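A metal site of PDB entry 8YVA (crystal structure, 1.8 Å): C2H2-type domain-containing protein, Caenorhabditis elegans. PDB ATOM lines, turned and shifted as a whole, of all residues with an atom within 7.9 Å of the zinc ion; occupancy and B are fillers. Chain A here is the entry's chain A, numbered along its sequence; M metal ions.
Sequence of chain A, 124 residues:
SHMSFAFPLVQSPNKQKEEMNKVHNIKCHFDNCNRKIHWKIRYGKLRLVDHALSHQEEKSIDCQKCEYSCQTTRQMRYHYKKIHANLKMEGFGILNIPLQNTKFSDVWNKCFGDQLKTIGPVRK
The zinc ion is bound by NE2 of His 84 (2.0 Å), NE2 of His 79 (2.1 Å), SG of Cys 63 (2.2 Å) and SG of Cys 66 (2.3 Å). The zinc ion has four donor atoms within binding distance.
The backbone NH of Cys 63 lies within hydrogen-bond range of the backbone carbonyl oxygen of Tyr 68, 2.9 Å away. N of Tyr 68 lies close to SG of Cys 66, at 3.5 Å. SG of Cys 63 sits close to N of Lys 65, at 3.3 Å.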
ATOM      1  N   ASP A  62      20.306 -20.359  30.811  1.00  0.00           N
ATOM      2  CA  ASP A  62      20.931 -21.399  29.987  1.00  0.00           C
ATOM      3  C   ASP A  62      20.258 -21.495  28.621  1.00  0.00           C
ATOM      4  O   ASP A  62      19.029 -21.534  28.533  1.00  0.00           O
ATOM      5  CB  ASP A  62      20.857 -22.760  30.671  1.00  0.00           C
ATOM      6  CG  ASP A  62      21.706 -22.841  31.930  1.00  0.00           C
ATOM      7  OD1 ASP A  62      22.838 -22.302  31.934  1.00  0.00           O
ATOM      8  OD2 ASP A  62      21.254 -23.442  32.917  1.00  0.00           O
ATOM      9  N   CYS A  63      21.061 -21.572  27.560  1.00  0.00           N
ATOM     10  CA  CYS A  63      20.509 -21.751  26.221  1.00  0.00           C
ATOM     11  C   CYS A  63      19.842 -23.123  26.117  1.00  0.00           C
ATOM     12  O   CYS A  63      20.294 -24.100  26.713  1.00  0.00           O
ATOM     13  CB  CYS A  63      21.607 -21.604  25.174  1.00  0.00           C
ATOM     14  SG  CYS A  63      21.022 -21.739  23.450  1.00  0.00           S
ATOM     15  N   GLN A  64      18.751 -23.195  25.352  1.00  0.00           N
ATOM     16  CA  GLN A  64      18.073 -24.471  25.131  1.00  0.00           C
ATOM     17  C   GLN A  64      18.675 -25.282  23.990  1.00  0.00           C
ATOM     18  O   GLN A  64      18.242 -26.421  23.786  1.00  0.00           O
ATOM     19  CB  GLN A  64      16.588 -24.265  24.840  1.00  0.00           C
ATOM     20  CG  GLN A  64      15.905 -23.204  25.699  1.00  0.00           C
ATOM     21  CD  GLN A  64      15.282 -23.776  26.948  1.00  0.00           C
ATOM     22  OE1 GLN A  64      15.829 -24.693  27.570  1.00  0.00           O
ATOM     23  NE2 GLN A  64      14.138 -23.226  27.338  1.00  0.00           N
ATOM     24  N   LYS A  65      19.643 -24.737  23.247  1.00  0.00           N
ATOM     25  CA  LYS A  65      20.226 -25.413  22.095  1.00  0.00           C
ATOM     26  C   LYS A  65      21.710 -25.723  22.229  1.00  0.00           C
ATOM     27  O   LYS A  65      22.162 -26.724  21.669  1.00  0.00           O
ATOM     28  CB  LYS A  65      20.033 -24.586  20.815  1.00  0.00           C
ATOM     29  CG  LYS A  65      18.697 -23.853  20.729  1.00  0.00           C
ATOM     30  CD  LYS A  65      17.563 -24.829  20.513  1.00  0.00           C
ATOM     31  CE  LYS A  65      16.228 -24.106  20.329  1.00  0.00           C
ATOM     32  NZ  LYS A  65      15.260 -24.979  19.619  1.00  0.00           N
ATOM     33  N   CYS A  66      22.490 -24.891  22.928  1.00  0.00           N
ATOM     34  CA  CYS A  66      23.921 -25.131  23.021  1.00  0.00           C
ATOM     35  C   CYS A  66      24.358 -24.908  24.466  1.00  0.00           C
ATOM     36  O   CYS A  66      23.534 -24.783  25.377  1.00  0.00           O
ATOM     37  CB  CYS A  66      24.678 -24.252  22.001  1.00  0.00           C
ATOM     38  SG  CYS A  66      24.828 -22.483  22.432  1.00  0.00           S
ATOM     39  N   GLU A  67      25.683 -24.893  24.672  1.00  0.00           N
ATOM     40  CA  GLU A  67      26.252 -24.795  26.015  1.00  0.00           C
ATOM     41  C   GLU A  67      26.192 -23.394  26.610  1.00  0.00           C
ATOM     42  O   GLU A  67      26.522 -23.235  27.794  1.00  0.00           O
ATOM     43  CB  GLU A  67      27.711 -25.286  25.989  1.00  0.00           C
ATOM     44  N   TYR A  68      25.768 -22.396  25.845  1.00  0.00           N
ATOM     45  CA  TYR A  68      25.875 -21.005  26.278  1.00  0.00           C
ATOM     46  C   TYR A  68      25.044 -20.723  27.526  1.00  0.00           C
ATOM     47  O   TYR A  68      23.935 -21.236  27.676  1.00  0.00           O
ATOM     48  CB  TYR A  68      25.401 -20.096  25.143  1.00  0.00           C
ATOM     49  CG  TYR A  68      25.577 -18.621  25.405  1.00  0.00           C
ATOM     50  CD1 TYR A  68      26.840 -18.050  25.398  1.00  0.00           C
ATOM     51  CD2 TYR A  68      24.481 -17.803  25.626  1.00  0.00           C
ATOM     52  CE1 TYR A  68      27.005 -16.695  25.623  1.00  0.00           C
ATOM     53  CE2 TYR A  68      24.641 -16.451  25.860  1.00  0.00           C
ATOM     54  CZ  TYR A  68      25.895 -15.903  25.852  1.00  0.00           C
ATOM     55  OH  TYR A  68      26.062 -14.558  26.075  1.00  0.00           O
ATOM     56  N   SER A  69      25.571 -19.876  28.412  1.00  0.00           N
ATOM     57  CA  SER A  69      24.825 -19.352  29.553  1.00  0.00           C
ATOM     58  C   SER A  69      25.178 -17.885  29.754  1.00  0.00           C
ATOM     59  O   SER A  69      26.256 -17.430  29.352  1.00  0.00           O
ATOM     60  CB  SER A  69      25.116 -20.164  30.821  1.00  0.00           C
ATOM     61  OG  SER A  69      26.437 -19.928  31.269  1.00  0.00           O
ATOM     62  N   MET A  76      20.448 -13.436  26.334  1.00  0.00           N
ATOM     63  CA  MET A  76      20.078 -14.670  25.665  1.00  0.00           C
ATOM     64  C   MET A  76      19.363 -14.397  24.344  1.00  0.00           C
ATOM     65  O   MET A  76      19.563 -15.117  23.370  1.00  0.00           O
ATOM     66  CB  MET A  76      19.227 -15.558  26.570  1.00  0.00           C
ATOM     67  CG  MET A  76      18.903 -16.873  25.840  1.00  0.00           C
ATOM     68  SD  MET A  76      20.380 -17.889  25.642  1.00  0.00           S
ATOM     69  CE  MET A  76      20.868 -18.172  27.348  1.00  0.00           C
ATOM     70  N   HIS A  79      21.970 -13.716  21.919  1.00  0.00           N
ATOM     71  CA  HIS A  79      22.619 -14.971  21.585  1.00  0.00           C
ATOM     72  C   HIS A  79      21.823 -15.739  20.528  1.00  0.00           C
ATOM     73  O   HIS A  79      22.389 -16.214  19.544  1.00  0.00           O
ATOM     74  CB  HIS A  79      22.808 -15.796  22.851  1.00  0.00           C
ATOM     75  CG  HIS A  79      23.251 -17.212  22.598  1.00  0.00           C
ATOM     76  ND1 HIS A  79      24.530 -17.524  22.174  1.00  0.00           N
ATOM     77  CD2 HIS A  79      22.592 -18.390  22.720  1.00  0.00           C
ATOM     78  CE1 HIS A  79      24.633 -18.835  22.042  1.00  0.00           C
ATOM     79  NE2 HIS A  79      23.466 -19.375  22.352  1.00  0.00           N
ATOM     80  N   TYR A  80      20.506 -15.860  20.721  1.00  0.00           N
ATOM     81  CA  TYR A  80      19.708 -16.618  19.763  1.00  0.00           C
ATOM     82  C   TYR A  80      19.713 -15.946  18.396  1.00  0.00           C
ATOM     83  O   TYR A  80      19.768 -16.625  17.366  1.00  0.00           O
ATOM     84  CB  TYR A  80      18.276 -16.766  20.253  1.00  0.00           C
ATOM     85  CG  TYR A  80      17.987 -18.022  21.045  1.00  0.00           C
ATOM     86  CD1 TYR A  80      18.506 -18.196  22.326  1.00  0.00           C
ATOM     87  CD2 TYR A  80      17.194 -19.029  20.518  1.00  0.00           C
ATOM     88  CE1 TYR A  80      18.227 -19.331  23.058  1.00  0.00           C
ATOM     89  CE2 TYR A  80      16.922 -20.171  21.239  1.00  0.00           C
ATOM     90  CZ  TYR A  80      17.430 -20.315  22.513  1.00  0.00           C
ATOM     91  OH  TYR A  80      17.165 -21.446  23.242  1.00  0.00           O
ATOM     92  N   ILE A  83      23.456 -16.674  16.989  1.00  0.00           N
ATOM     93  CA  ILE A  83      23.946 -18.052  16.906  1.00  0.00           C
ATOM     94  C   ILE A  83      22.860 -19.002  16.427  1.00  0.00           C
ATOM     95  O   ILE A  83      23.148 -20.012  15.772  1.00  0.00           O
ATOM     96  CB  ILE A  83      24.516 -18.494  18.267  1.00  0.00           C
ATOM     97  CG1 ILE A  83      25.590 -17.513  18.739  1.00  0.00           C
ATOM     98  CG2 ILE A  83      25.086 -19.907  18.192  1.00  0.00           C
ATOM     99  CD1 ILE A  83      26.738 -17.327  17.757  1.00  0.00           C
ATOM    100  N   HIS A  84      21.600 -18.721  16.766  1.00  0.00           N
ATOM    101  CA  HIS A  84      20.498 -19.616  16.404  1.00  0.00           C
ATOM    102  C   HIS A  84      19.471 -18.879  15.561  1.00  0.00           C
ATOM    103  O   HIS A  84      18.272 -18.835  15.900  1.00  0.00           O
ATOM    104  CB  HIS A  84      19.852 -20.197  17.673  1.00  0.00           C
ATOM    105  CG  HIS A  84      20.833 -20.812  18.630  1.00  0.00           C
ATOM    106  ND1 HIS A  84      21.616 -21.900  18.296  1.00  0.00           N
ATOM    107  CD2 HIS A  84      21.150 -20.498  19.908  1.00  0.00           C
ATOM    108  CE1 HIS A  84      22.379 -22.215  19.330  1.00  0.00           C
ATOM    109  NE2 HIS A  84      22.108 -21.390  20.325  1.00  0.00           N
HETATM  110 ZN    ZN M   1      22.830 -21.365  22.171  1.00  0.00          ZN
